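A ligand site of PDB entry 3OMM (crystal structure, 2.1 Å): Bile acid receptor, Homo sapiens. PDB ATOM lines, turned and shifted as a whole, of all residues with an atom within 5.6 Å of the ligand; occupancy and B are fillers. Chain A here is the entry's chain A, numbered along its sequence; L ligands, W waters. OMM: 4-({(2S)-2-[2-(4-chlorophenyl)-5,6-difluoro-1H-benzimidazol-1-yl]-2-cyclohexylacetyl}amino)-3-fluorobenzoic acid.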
ATOM      1  N   GLN A  24     -25.643 -21.536 -22.384  1.00  0.00           N
ATOM      2  CA  GLN A  24     -25.205 -20.761 -21.237  1.00  0.00           C
ATOM      3  C   GLN A  24     -23.729 -20.527 -21.207  1.00  0.00           C
ATOM      4  O   GLN A  24     -22.972 -21.357 -21.703  1.00  0.00           O
ATOM      5  CB  GLN A  24     -25.589 -21.488 -19.958  1.00  0.00           C
ATOM      6  CG  GLN A  24     -26.844 -20.920 -19.363  1.00  0.00           C
ATOM      7  CD  GLN A  24     -27.242 -21.666 -18.139  1.00  0.00           C
ATOM      8  OE1 GLN A  24     -27.730 -21.074 -17.185  1.00  0.00           O
ATOM      9  NE2 GLN A  24     -27.069 -22.974 -18.161  1.00  0.00           N
ATOM     10  N   ARG A  25     -23.331 -19.424 -20.531  1.00  0.00           N
ATOM     11  CA  ARG A  25     -21.928 -19.077 -20.331  1.00  0.00           C
ATOM     12  C   ARG A  25     -21.208 -20.262 -19.770  1.00  0.00           C
ATOM     13  O   ARG A  25     -21.697 -20.912 -18.824  1.00  0.00           O
ATOM     14  CB  ARG A  25     -21.754 -17.867 -19.410  1.00  0.00           C
ATOM     15  CG  ARG A  25     -22.001 -16.556 -20.088  1.00  0.00           C
ATOM     16  CD  ARG A  25     -20.968 -15.528 -19.721  1.00  0.00           C
ATOM     17  NE  ARG A  25     -21.315 -14.227 -20.315  1.00  0.00           N
ATOM     18  CZ  ARG A  25     -21.347 -13.082 -19.634  1.00  0.00           C
ATOM     19  NH1 ARG A  25     -20.997 -13.033 -18.355  1.00  0.00           N
ATOM     20  NH2 ARG A  25     -21.700 -11.959 -20.256  1.00  0.00           N
ATOM     21  N   ILE A  30     -16.270 -18.214 -15.965  1.00  0.00           N
ATOM     22  CA  ILE A  30     -16.585 -17.668 -14.631  1.00  0.00           C
ATOM     23  C   ILE A  30     -15.463 -17.976 -13.621  1.00  0.00           C
ATOM     24  O   ILE A  30     -14.939 -17.047 -13.012  1.00  0.00           O
ATOM     25  CB  ILE A  30     -17.998 -18.192 -14.166  1.00  0.00           C
ATOM     26  CG1 ILE A  30     -19.151 -17.612 -15.047  1.00  0.00           C
ATOM     27  CG2 ILE A  30     -18.268 -17.912 -12.683  1.00  0.00           C
ATOM     28  CD1 ILE A  30     -19.752 -18.555 -16.020  1.00  0.00           C
ATOM     29  N   THR A  31     -15.124 -19.270 -13.428  1.00  0.00           N
ATOM     30  CA  THR A  31     -14.124 -19.703 -12.456  1.00  0.00           C
ATOM     31  C   THR A  31     -12.684 -19.374 -12.809  1.00  0.00           C
ATOM     32  O   THR A  31     -11.916 -19.080 -11.892  1.00  0.00           O
ATOM     33  CB  THR A  31     -14.313 -21.155 -12.020  1.00  0.00           C
ATOM     34  OG1 THR A  31     -14.190 -21.994 -13.152  1.00  0.00           O
ATOM     35  CG2 THR A  31     -15.637 -21.394 -11.340  1.00  0.00           C
ATOM     36  N   ILE A  34     -12.289 -15.728 -11.556  1.00  0.00           N
ATOM     37  CA  ILE A  34     -12.309 -15.601 -10.089  1.00  0.00           C
ATOM     38  C   ILE A  34     -10.988 -16.133  -9.510  1.00  0.00           C
ATOM     39  O   ILE A  34     -10.412 -15.516  -8.618  1.00  0.00           O
ATOM     40  CB  ILE A  34     -13.584 -16.247  -9.463  1.00  0.00           C
ATOM     41  CG1 ILE A  34     -14.855 -15.465  -9.881  1.00  0.00           C
ATOM     42  CG2 ILE A  34     -13.476 -16.335  -7.938  1.00  0.00           C
ATOM     43  CD1 ILE A  34     -16.189 -16.194  -9.759  1.00  0.00           C
ATOM     44  N   ASN A  44     -15.537  -7.045  -7.669  1.00  0.00           N
ATOM     45  CA  ASN A  44     -16.381  -8.227  -7.499  1.00  0.00           C
ATOM     46  C   ASN A  44     -17.857  -7.860  -7.562  1.00  0.00           C
ATOM     47  O   ASN A  44     -18.611  -8.567  -8.213  1.00  0.00           O
ATOM     48  CB  ASN A  44     -16.043  -8.951  -6.208  1.00  0.00           C
ATOM     49  CG  ASN A  44     -14.803  -9.773  -6.335  1.00  0.00           C
ATOM     50  OD1 ASN A  44     -14.541 -10.388  -7.377  1.00  0.00           O
ATOM     51  ND2 ASN A  44     -14.048  -9.868  -5.263  1.00  0.00           N
ATOM     52  N   ILE A  47     -18.510  -7.450 -11.217  1.00  0.00           N
ATOM     53  CA  ILE A  47     -18.523  -8.754 -11.894  1.00  0.00           C
ATOM     54  C   ILE A  47     -19.893  -9.383 -11.579  1.00  0.00           C
ATOM     55  O   ILE A  47     -20.587  -9.807 -12.485  1.00  0.00           O
ATOM     56  CB  ILE A  47     -17.302  -9.633 -11.459  1.00  0.00           C
ATOM     57  CG1 ILE A  47     -15.982  -8.987 -11.955  1.00  0.00           C
ATOM     58  CG2 ILE A  47     -17.420 -11.099 -11.975  1.00  0.00           C
ATOM     59  CD1 ILE A  47     -14.737  -9.504 -11.237  1.00  0.00           C
ATOM     60  N   LEU A  48     -20.331  -9.334 -10.328  1.00  0.00           N
ATOM     61  CA  LEU A  48     -21.635  -9.911  -9.925  1.00  0.00           C
ATOM     62  C   LEU A  48     -22.810  -9.327 -10.728  1.00  0.00           C
ATOM     63  O   LEU A  48     -23.618 -10.082 -11.239  1.00  0.00           O
ATOM     64  CB  LEU A  48     -21.865  -9.748  -8.419  1.00  0.00           C
ATOM     65  CG  LEU A  48     -23.279 -10.045  -7.855  1.00  0.00           C
ATOM     66  CD1 LEU A  48     -23.690 -11.509  -8.066  1.00  0.00           C
ATOM     67  CD2 LEU A  48     -23.367  -9.659  -6.402  1.00  0.00           C
ATOM     68  N   MET A  51     -22.597 -10.513 -14.516  1.00  0.00           N
ATOM     69  CA  MET A  51     -22.939 -11.940 -14.586  1.00  0.00           C
ATOM     70  C   MET A  51     -24.421 -12.125 -14.366  1.00  0.00           C
ATOM     71  O   MET A  51     -25.057 -12.895 -15.077  1.00  0.00           O
ATOM     72  CB  MET A  51     -22.222 -12.736 -13.483  1.00  0.00           C
ATOM     73  CG  MET A  51     -20.762 -12.784 -13.653  1.00  0.00           C
ATOM     74  SD  MET A  51     -20.228 -13.875 -14.970  1.00  0.00           S
ATOM     75  CE  MET A  51     -18.437 -13.799 -14.598  1.00  0.00           C
ATOM     76  N   ALA A  52     -24.967 -11.447 -13.318  1.00  0.00           N
ATOM     77  CA  ALA A  52     -26.385 -11.554 -12.957  1.00  0.00           C
ATOM     78  C   ALA A  52     -27.304 -11.003 -14.027  1.00  0.00           C
ATOM     79  O   ALA A  52     -28.353 -11.592 -14.237  1.00  0.00           O
ATOM     80  CB  ALA A  52     -26.651 -10.905 -11.599  1.00  0.00           C
ATOM     81  N   ASN A  54     -26.486 -10.848 -17.369  1.00  0.00           N
ATOM     82  CA  ASN A  54     -26.417 -11.828 -18.456  1.00  0.00           C
ATOM     83  C   ASN A  54     -27.202 -13.091 -18.110  1.00  0.00           C
ATOM     84  O   ASN A  54     -27.848 -13.662 -18.988  1.00  0.00           O
ATOM     85  CB  ASN A  54     -24.970 -12.206 -18.741  1.00  0.00           C
ATOM     86  CG  ASN A  54     -24.830 -13.310 -19.760  1.00  0.00           C
ATOM     87  OD1 ASN A  54     -24.588 -14.475 -19.400  1.00  0.00           O
ATOM     88  ND2 ASN A  54     -25.088 -13.014 -21.045  1.00  0.00           N
ATOM     89  N   HIS A  55     -27.152 -13.544 -16.825  1.00  0.00           N
ATOM     90  CA  HIS A  55     -27.888 -14.732 -16.408  1.00  0.00           C
ATOM     91  C   HIS A  55     -29.402 -14.597 -16.643  1.00  0.00           C
ATOM     92  O   HIS A  55     -30.022 -15.553 -17.116  1.00  0.00           O
ATOM     93  CB  HIS A  55     -27.613 -15.084 -14.924  1.00  0.00           C
ATOM     94  CG  HIS A  55     -28.351 -16.319 -14.509  1.00  0.00           C
ATOM     95  ND1 HIS A  55     -29.622 -16.244 -14.024  1.00  0.00           N
ATOM     96  CD2 HIS A  55     -27.996 -17.614 -14.642  1.00  0.00           C
ATOM     97  CE1 HIS A  55     -30.006 -17.506 -13.846  1.00  0.00           C
ATOM     98  NE2 HIS A  55     -29.059 -18.361 -14.212  1.00  0.00           N
ATOM     99  N   MET A  89     -30.484 -18.407 -10.529  1.00  0.00           N
ATOM    100  CA  MET A  89     -29.113 -17.857 -10.420  1.00  0.00           C
ATOM    101  C   MET A  89     -28.241 -18.615  -9.374  1.00  0.00           C
ATOM    102  O   MET A  89     -27.104 -18.979  -9.670  1.00  0.00           O
ATOM    103  CB  MET A  89     -29.178 -16.340 -10.200  1.00  0.00           C
ATOM    104  CG  MET A  89     -28.498 -15.831  -8.942  1.00  0.00           C
ATOM    105  SD  MET A  89     -26.764 -15.535  -9.212  1.00  0.00           S
ATOM    106  CE  MET A  89     -26.875 -14.526 -10.640  1.00  0.00           C
ATOM    107  N   PHE A  90     -28.791 -18.892  -8.185  1.00  0.00           N
ATOM    108  CA  PHE A  90     -28.107 -19.631  -7.132  1.00  0.00           C
ATOM    109  C   PHE A  90     -27.922 -21.056  -7.525  1.00  0.00           C
ATOM    110  O   PHE A  90     -26.909 -21.648  -7.167  1.00  0.00           O
ATOM    111  CB  PHE A  90     -28.864 -19.498  -5.793  1.00  0.00           C
ATOM    112  CG  PHE A  90     -28.565 -18.161  -5.141  1.00  0.00           C
ATOM    113  CD1 PHE A  90     -27.281 -17.866  -4.682  1.00  0.00           C
ATOM    114  CD2 PHE A  90     -29.522 -17.158  -5.115  1.00  0.00           C
ATOM    115  CE1 PHE A  90     -26.976 -16.618  -4.175  1.00  0.00           C
ATOM    116  CE2 PHE A  90     -29.218 -15.908  -4.595  1.00  0.00           C
ATOM    117  CZ  PHE A  90     -27.953 -15.653  -4.123  1.00  0.00           C
ATOM    118  N   ARG A  92     -27.544 -22.299 -10.602  1.00  0.00           N
ATOM    119  CA  ARG A  92     -26.470 -22.256 -11.577  1.00  0.00           C
ATOM    120  C   ARG A  92     -25.114 -21.948 -10.854  1.00  0.00           C
ATOM    121  O   ARG A  92     -24.088 -22.552 -11.186  1.00  0.00           O
ATOM    122  CB  ARG A  92     -26.791 -21.200 -12.639  1.00  0.00           C
ATOM    123  CG  ARG A  92     -25.690 -21.014 -13.696  1.00  0.00           C
ATOM    124  CD  ARG A  92     -25.378 -22.307 -14.444  1.00  0.00           C
ATOM    125  NE  ARG A  92     -24.325 -22.086 -15.443  1.00  0.00           N
ATOM    126  CZ  ARG A  92     -24.005 -22.955 -16.387  1.00  0.00           C
ATOM    127  NH1 ARG A  92     -24.656 -24.102 -16.487  1.00  0.00           N
ATOM    128  NH2 ARG A  92     -23.058 -22.681 -17.260  1.00  0.00           N
ATOM    129  N   SER A  93     -25.117 -21.063  -9.846  1.00  0.00           N
ATOM    130  CA  SER A  93     -23.893 -20.774  -9.052  1.00  0.00           C
ATOM    131  C   SER A  93     -23.445 -22.045  -8.288  1.00  0.00           C
ATOM    132  O   SER A  93     -22.248 -22.357  -8.239  1.00  0.00           O
ATOM    133  CB  SER A  93     -24.151 -19.649  -8.075  1.00  0.00           C
ATOM    134  OG  SER A  93     -24.222 -18.388  -8.721  1.00  0.00           O
ATOM    135  N   ALA A  94     -24.416 -22.803  -7.733  1.00  0.00           N
ATOM    136  CA  ALA A  94     -24.163 -24.069  -7.031  1.00  0.00           C
ATOM    137  C   ALA A  94     -23.556 -25.089  -7.985  1.00  0.00           C
ATOM    138  O   ALA A  94     -22.590 -25.734  -7.621  1.00  0.00           O
ATOM    139  CB  ALA A  94     -25.460 -24.602  -6.427  1.00  0.00           C
ATOM    140  N   ILE A  96     -21.821 -24.498 -10.873  1.00  0.00           N
ATOM    141  CA  ILE A  96     -20.472 -24.023 -11.169  1.00  0.00           C
ATOM    142  C   ILE A  96     -19.519 -24.275 -10.000  1.00  0.00           C
ATOM    143  O   ILE A  96     -18.398 -24.696 -10.246  1.00  0.00           O
ATOM    144  CB  ILE A  96     -20.503 -22.564 -11.640  1.00  0.00           C
ATOM    145  CG1 ILE A  96     -21.222 -22.494 -13.001  1.00  0.00           C
ATOM    146  CG2 ILE A  96     -19.093 -21.951 -11.730  1.00  0.00           C
ATOM    147  CD1 ILE A  96     -21.329 -21.145 -13.587  1.00  0.00           C
ATOM    148  N   PHE A  97     -19.970 -24.043  -8.772  1.00  0.00           N
ATOM    149  CA  PHE A  97     -19.190 -24.258  -7.555  1.00  0.00           C
ATOM    150  C   PHE A  97     -18.760 -25.726  -7.373  1.00  0.00           C
ATOM    151  O   PHE A  97     -17.640 -25.966  -6.921  1.00  0.00           O
ATOM    152  CB  PHE A  97     -19.954 -23.789  -6.316  1.00  0.00           C
ATOM    153  CG  PHE A  97     -19.134 -23.769  -5.042  1.00  0.00           C
ATOM    154  CD1 PHE A  97     -18.221 -22.743  -4.806  1.00  0.00           C
ATOM    155  CD2 PHE A  97     -19.274 -24.769  -4.092  1.00  0.00           C
ATOM    156  CE1 PHE A  97     -17.471 -22.720  -3.634  1.00  0.00           C
ATOM    157  CE2 PHE A  97     -18.499 -24.765  -2.932  1.00  0.00           C
ATOM    158  CZ  PHE A  97     -17.606 -23.729  -2.704  1.00  0.00           C
ATOM    159  N   ASN A  98     -19.649 -26.674  -7.690  1.00  0.00           N
ATOM    160  CA  ASN A  98     -19.343 -28.090  -7.488  1.00  0.00           C
ATOM    161  C   ASN A  98     -18.757 -28.788  -8.697  1.00  0.00           C
ATOM    162  O   ASN A  98     -18.653 -30.015  -8.660  1.00  0.00           O
ATOM    163  CB  ASN A  98     -20.535 -28.853  -6.924  1.00  0.00           C
ATOM    164  CG  ASN A  98     -20.947 -28.361  -5.585  1.00  0.00           C
ATOM    165  OD1 ASN A  98     -20.332 -28.673  -4.546  1.00  0.00           O
ATOM    166  ND2 ASN A  98     -22.003 -27.578  -5.576  1.00  0.00           N
ATOM    167  N   LEU A 109     -11.303 -21.102  -4.976  1.00  0.00           N
ATOM    168  CA  LEU A 109     -12.566 -20.539  -5.465  1.00  0.00           C
ATOM    169  C   LEU A 109     -13.456 -20.207  -4.282  1.00  0.00           C
ATOM    170  O   LEU A 109     -14.007 -19.109  -4.229  1.00  0.00           O
ATOM    171  CB  LEU A 109     -13.256 -21.528  -6.420  1.00  0.00           C
ATOM    172  CG  LEU A 109     -14.605 -21.114  -7.057  1.00  0.00           C
ATOM    173  CD1 LEU A 109     -14.435 -19.917  -7.981  1.00  0.00           C
ATOM    174  CD2 LEU A 109     -15.243 -22.284  -7.752  1.00  0.00           C
ATOM    175  N   ILE A 113     -14.700 -16.434  -3.152  1.00  0.00           N
ATOM    176  CA  ILE A 113     -16.119 -16.056  -3.008  1.00  0.00           C
ATOM    177  C   ILE A 113     -16.416 -15.527  -1.579  1.00  0.00           C
ATOM    178  O   ILE A 113     -17.118 -14.536  -1.423  1.00  0.00           O
ATOM    179  CB  ILE A 113     -17.061 -17.215  -3.464  1.00  0.00           C
ATOM    180  CG1 ILE A 113     -16.883 -17.541  -4.965  1.00  0.00           C
ATOM    181  CG2 ILE A 113     -18.547 -16.916  -3.141  1.00  0.00           C
ATOM    182  CD1 ILE A 113     -17.237 -18.893  -5.317  1.00  0.00           C
ATOM    183  N   SER A 116     -15.245 -11.990  -1.290  1.00  0.00           N
ATOM    184  CA  SER A 116     -15.629 -11.194  -2.463  1.00  0.00           C
ATOM    185  C   SER A 116     -16.280  -9.850  -2.108  1.00  0.00           C
ATOM    186  O   SER A 116     -16.376  -8.979  -2.976  1.00  0.00           O
ATOM    187  CB  SER A 116     -16.562 -12.004  -3.375  1.00  0.00           C
ATOM    188  OG  SER A 116     -17.838 -12.163  -2.761  1.00  0.00           O
ATOM    189  N   ILE A 118     -19.324  -9.989  -0.109  1.00  0.00           N
ATOM    190  CA  ILE A 118     -20.610 -10.442   0.435  1.00  0.00           C
ATOM    191  C   ILE A 118     -20.544 -10.388   1.992  1.00  0.00           C
ATOM    192  O   ILE A 118     -19.498 -10.702   2.565  1.00  0.00           O
ATOM    193  CB  ILE A 118     -20.949 -11.878  -0.076  1.00  0.00           C
ATOM    194  CG1 ILE A 118     -22.177 -12.481   0.603  1.00  0.00           C
ATOM    195  CG2 ILE A 118     -19.758 -12.812   0.073  1.00  0.00           C
ATOM    196  CD1 ILE A 118     -23.477 -11.800   0.319  1.00  0.00           C
ATOM    197  N   MET A 126     -25.346 -19.740   2.165  1.00  0.00           N
ATOM    198  CA  MET A 126     -24.934 -19.919   0.773  1.00  0.00           C
ATOM    199  C   MET A 126     -24.033 -21.115   0.569  1.00  0.00           C
ATOM    200  O   MET A 126     -24.338 -21.956  -0.266  1.00  0.00           O
ATOM    201  CB  MET A 126     -24.280 -18.647   0.244  1.00  0.00           C
ATOM    202  CG  MET A 126     -23.952 -18.719  -1.207  1.00  0.00           C
ATOM    203  SD  MET A 126     -22.856 -17.383  -1.683  1.00  0.00           S
ATOM    204  CE  MET A 126     -24.009 -16.038  -1.541  1.00  0.00           C
ATOM    205  N   TYR A 130     -24.730 -24.563  -1.316  1.00  0.00           N
ATOM    206  CA  TYR A 130     -23.870 -25.079  -2.390  1.00  0.00           C
ATOM    207  C   TYR A 130     -23.344 -26.458  -2.038  1.00  0.00           C
ATOM    208  O   TYR A 130     -23.194 -27.295  -2.927  1.00  0.00           O
ATOM    209  CB  TYR A 130     -22.684 -24.154  -2.726  1.00  0.00           C
ATOM    210  CG  TYR A 130     -23.014 -22.769  -3.266  1.00  0.00           C
ATOM    211  CD1 TYR A 130     -24.266 -22.455  -3.745  1.00  0.00           C
ATOM    212  CD2 TYR A 130     -22.015 -21.787  -3.343  1.00  0.00           C
ATOM    213  CE1 TYR A 130     -24.573 -21.180  -4.235  1.00  0.00           C
ATOM    214  CE2 TYR A 130     -22.305 -20.518  -3.832  1.00  0.00           C
ATOM    215  CZ  TYR A 130     -23.582 -20.219  -4.295  1.00  0.00           C
ATOM    216  OH  TYR A 130     -23.887 -18.944  -4.735  1.00  0.00           O
ATOM    217  N   HIS A 208     -32.559 -11.981  -0.872  1.00  0.00           N
ATOM    218  CA  HIS A 208     -31.789 -11.668  -2.089  1.00  0.00           C
ATOM    219  C   HIS A 208     -31.440 -10.173  -2.262  1.00  0.00           C
ATOM    220  O   HIS A 208     -30.306  -9.849  -2.601  1.00  0.00           O
ATOM    221  CB  HIS A 208     -32.438 -12.253  -3.358  1.00  0.00           C
ATOM    222  CG  HIS A 208     -33.743 -11.626  -3.749  1.00  0.00           C
ATOM    223  ND1 HIS A 208     -34.958 -12.231  -3.448  1.00  0.00           N
ATOM    224  CD2 HIS A 208     -33.992 -10.501  -4.461  1.00  0.00           C
ATOM    225  CE1 HIS A 208     -35.892 -11.438  -3.943  1.00  0.00           C
ATOM    226  NE2 HIS A 208     -35.353 -10.374  -4.563  1.00  0.00           N
ATOM    227  N   MET A 211     -28.781  -9.180   0.156  1.00  0.00           N
ATOM    228  CA  MET A 211     -27.495  -9.782  -0.169  1.00  0.00           C
ATOM    229  C   MET A 211     -26.699  -8.871  -1.091  1.00  0.00           C
ATOM    230  O   MET A 211     -25.482  -8.802  -0.975  1.00  0.00           O
ATOM    231  CB  MET A 211     -27.690 -11.141  -0.837  1.00  0.00           C
ATOM    232  CG  MET A 211     -27.638 -12.281   0.121  1.00  0.00           C
ATOM    233  SD  MET A 211     -27.839 -13.868  -0.731  1.00  0.00           S
ATOM    234  CE  MET A 211     -29.577 -14.141  -0.471  1.00  0.00           C
ATOM    235  N   LEU A 212     -27.401  -8.178  -1.995  1.00  0.00           N
ATOM    236  CA  LEU A 212     -26.763  -7.238  -2.882  1.00  0.00           C
ATOM    237  C   LEU A 212     -26.507  -5.921  -2.144  1.00  0.00           C
ATOM    238  O   LEU A 212     -25.424  -5.375  -2.284  1.00  0.00           O
ATOM    239  CB  LEU A 212     -27.616  -6.994  -4.133  1.00  0.00           C
ATOM    240  CG  LEU A 212     -28.011  -8.222  -5.014  1.00  0.00           C
ATOM    241  CD1 LEU A 212     -28.678  -7.744  -6.297  1.00  0.00           C
ATOM    242  CD2 LEU A 212     -26.813  -9.078  -5.396  1.00  0.00           C
ATOM    243  N   TRP A 215     -23.481  -5.699   0.360  1.00  0.00           N
ATOM    244  CA  TRP A 215     -22.146  -5.967  -0.185  1.00  0.00           C
ATOM    245  C   TRP A 215     -21.250  -4.812   0.292  1.00  0.00           C
ATOM    246  O   TRP A 215     -21.695  -3.660   0.284  1.00  0.00           O
ATOM    247  CB  TRP A 215     -22.172  -5.987  -1.716  1.00  0.00           C
ATOM    248  CG  TRP A 215     -21.069  -6.787  -2.320  1.00  0.00           C
ATOM    249  CD1 TRP A 215     -19.820  -6.350  -2.664  1.00  0.00           C
ATOM    250  CD2 TRP A 215     -21.159  -8.150  -2.763  1.00  0.00           C
ATOM    251  NE1 TRP A 215     -19.123  -7.361  -3.288  1.00  0.00           N
ATOM    252  CE2 TRP A 215     -19.927  -8.469  -3.375  1.00  0.00           C
ATOM    253  CE3 TRP A 215     -22.174  -9.115  -2.732  1.00  0.00           C
ATOM    254  CZ2 TRP A 215     -19.666  -9.741  -3.906  1.00  0.00           C
ATOM    255  CZ3 TRP A 215     -21.910 -10.373  -3.243  1.00  0.00           C
ATOM    256  CH2 TRP A 215     -20.675 -10.676  -3.822  1.00  0.00           C
ATOM    257  N   TRP A 230     -34.292  -8.400  -9.219  1.00  0.00           N
ATOM    258  CA  TRP A 230     -33.941  -8.491  -7.809  1.00  0.00           C
ATOM    259  C   TRP A 230     -34.810  -7.405  -7.241  1.00  0.00           C
ATOM    260  O   TRP A 230     -35.563  -6.781  -7.996  1.00  0.00           O
ATOM    261  CB  TRP A 230     -32.424  -8.280  -7.596  1.00  0.00           C
ATOM    262  CG  TRP A 230     -31.583  -9.367  -8.214  1.00  0.00           C
ATOM    263  CD1 TRP A 230     -31.407  -9.623  -9.532  1.00  0.00           C
ATOM    264  CD2 TRP A 230     -30.830 -10.383  -7.517  1.00  0.00           C
ATOM    265  NE1 TRP A 230     -30.596 -10.714  -9.715  1.00  0.00           N
ATOM    266  CE2 TRP A 230     -30.213 -11.184  -8.497  1.00  0.00           C
ATOM    267  CE3 TRP A 230     -30.615 -10.680  -6.147  1.00  0.00           C
ATOM    268  CZ2 TRP A 230     -29.345 -12.237  -8.163  1.00  0.00           C
ATOM    269  CZ3 TRP A 230     -29.763 -11.730  -5.829  1.00  0.00           C
ATOM    270  CH2 TRP A 230     -29.163 -12.511  -6.826  1.00  0.00           C
HETATM  271  N1  OMM L   1     -21.287 -16.430  -7.652  1.00  0.00           N
HETATM  272  C2  OMM L   1     -22.033 -16.666  -6.515  1.00  0.00           C
HETATM  273  N3  OMM L   1     -21.808 -17.868  -6.079  1.00  0.00           N
HETATM  274  C4  OMM L   1     -20.583 -17.567  -7.896  1.00  0.00           C
HETATM  275  C5  OMM L   1     -20.919 -18.483  -6.883  1.00  0.00           C
HETATM  276  C6  OMM L   1     -21.584 -15.442  -9.852  1.00  0.00           C
HETATM  277  C7  OMM L   1     -21.236 -15.175  -8.415  1.00  0.00           C
HETATM  278  C8  OMM L   1     -19.661 -17.890  -8.886  1.00  0.00           C
HETATM  279  N9  OMM L   1     -22.545 -16.371 -10.095  1.00  0.00           N
HETATM  280  C10 OMM L   1     -20.319 -19.742  -6.880  1.00  0.00           C
HETATM  281  C11 OMM L   1     -19.074 -19.130  -8.864  1.00  0.00           C
HETATM  282  C12 OMM L   1     -22.950 -16.798 -11.356  1.00  0.00           C
HETATM  283  C13 OMM L   1     -24.100 -18.063 -15.304  1.00  0.00           C
HETATM  284  C14 OMM L   1     -22.977 -15.680  -5.944  1.00  0.00           C
HETATM  285  C15 OMM L   1     -19.426 -20.044  -7.881  1.00  0.00           C
HETATM  286  C16 OMM L   1     -23.677 -17.634 -13.936  1.00  0.00           C
HETATM  287  C17 OMM L   1     -23.759 -16.001 -12.155  1.00  0.00           C
HETATM  288  C18 OMM L   1     -24.120 -16.404 -13.425  1.00  0.00           C
HETATM  289  O19 OMM L   1     -21.001 -14.849 -10.753  1.00  0.00           O
HETATM  290  O20 OMM L   1     -24.793 -17.324 -15.943  1.00  0.00           O
HETATM  291  C21 OMM L   1     -22.491 -18.033 -11.865  1.00  0.00           C
HETATM  292  C22 OMM L   1     -22.892 -18.447 -13.121  1.00  0.00           C
HETATM  293  C23 OMM L   1     -19.842 -14.516  -8.227  1.00  0.00           C
HETATM  294  C24 OMM L   1     -22.650 -15.037  -4.755  1.00  0.00           C
HETATM  295  C25 OMM L   1     -24.111 -15.293  -6.657  1.00  0.00           C
HETATM  296  F26 OMM L   1     -18.175 -19.421  -9.823  1.00  0.00           F
HETATM  297  F27 OMM L   1     -18.844 -21.248  -7.898  1.00  0.00           F
HETATM  298  F28 OMM L   1     -24.119 -14.788 -11.698  1.00  0.00           F
HETATM  299  O29 OMM L   1     -23.764 -19.252 -15.837  1.00  0.00           O
HETATM  300  C30 OMM L   1     -24.657 -13.731  -4.922  1.00  0.00           C
HETATM  301  C31 OMM L   1     -24.939 -14.302  -6.155  1.00  0.00           C
HETATM  302  C32 OMM L   1     -23.497 -14.087  -4.255  1.00  0.00           C
HETATM  303 CL33 OMM L   1     -25.696 -12.505  -4.234  1.00  0.00          CL
HETATM  304  C34 OMM L   1     -19.872 -13.060  -8.725  1.00  0.00           C
HETATM  305  C35 OMM L   1     -19.479 -14.516  -6.741  1.00  0.00           C
HETATM  306  C36 OMM L   1     -18.083 -13.890  -6.549  1.00  0.00           C
HETATM  307  C37 OMM L   1     -18.525 -12.348  -8.481  1.00  0.00           C
HETATM  308  C38 OMM L   1     -18.181 -12.422  -6.980  1.00  0.00           C
HETATM  309  O   HOH W   1     -26.124 -18.518 -17.738  1.00  0.00           O
HETATM  310  O   HOH W   2     -23.721 -14.894 -16.921  1.00  0.00           O
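A nitrogen (N3) of the ligand sits at hydrogen-bond distance from the side-chain hydroxyl (OH) of Tyr 130, 2.7 Å away. OG of Ser 93 lies within hydrogen-bond range of N9 of the ligand, 3.0 Å away. O29 of the ligand is in salt-bridge range of NE of Arg 92 (2.9 Å).
The side-chain amide nitrogen (ND2) of Asn 44 sits close to the backbone carbonyl oxygen (O) of Ser 116 (3.4 Å). O of Arg 25 is in hydrogen-bond range of NH2 of Arg 92 (2.7 Å). The side-chain sulfur (SD) of Met 51 sits at hydrogen-bond distance from the guanidinium group (NH1) of Arg 25, 3.6 Å away. The guanidinium group of Arg 92 sits close to the side-chain amide nitrogen of Gln 24, 3.1 Å away. The side-chain hydroxyl of Ser 116 lies within hydrogen-bond range of the backbone carbonyl oxygen of Ile 113 (2.8 Å). The side-chain hydroxyl (OG) of Ser 93 sits at hydrogen-bond distance from the backbone carbonyl oxygen (O) of Met 89, at 3.1 Å. The backbone carbonyl oxygen (O) of Tyr 130 lies within hydrogen-bond range of the side-chain amide nitrogen (ND2) of Asn 98 (2.9 Å). O of Ser 116 sits at hydrogen-bond distance from NE1 of Trp 215 (3.2 Å).
F28 of the ligand lies close to SD of Met 89 (3.7 Å). The backbone NH (N) of Phe 97 sits close to a fluorine (F27) of the ligand (3.1 Å). Residues that only touch the ligand: Ile 96 (3.2 Å), Ile 30 (3.2 Å), Met 51 (3.3 Å), Met 126 (3.4 Å), His 55 (3.5 Å), Thr 31 (3.6 Å), Ile 113 (3.6 Å), Leu 48 (3.6 Å), Phe 90 (3.7 Å), Leu 109 (3.7 Å), Leu 212 (3.8 Å), Ile 34 (3.8 Å), Asn 44 (3.8 Å), Ala 52 (3.8 Å), Ile 47 (3.9 Å), Ser 116 (3.97 Å) and Arg 25 (3.99 Å). Hydrophobic or aromatic side chains within 4 Å of the ligand: Ile 30, Ile 34, Ile 47, Leu 48, Met 51, His 55, Met 89, Phe 90, Ile 96, Phe 97, Leu 109, Ile 113, Met 126, Tyr 130 and Leu 212. Of the 31 residues printed, 22 come within 4 Å of the ligand.
Water W1 bridges O20 of the ligand and OE1 of Gln 24. Water W2 lies within hydrogen-bond range of OD1 of Asn 54 (2.7 Å), O20 of the ligand (2.8 Å) and O of Met 51 (3.0 Å).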
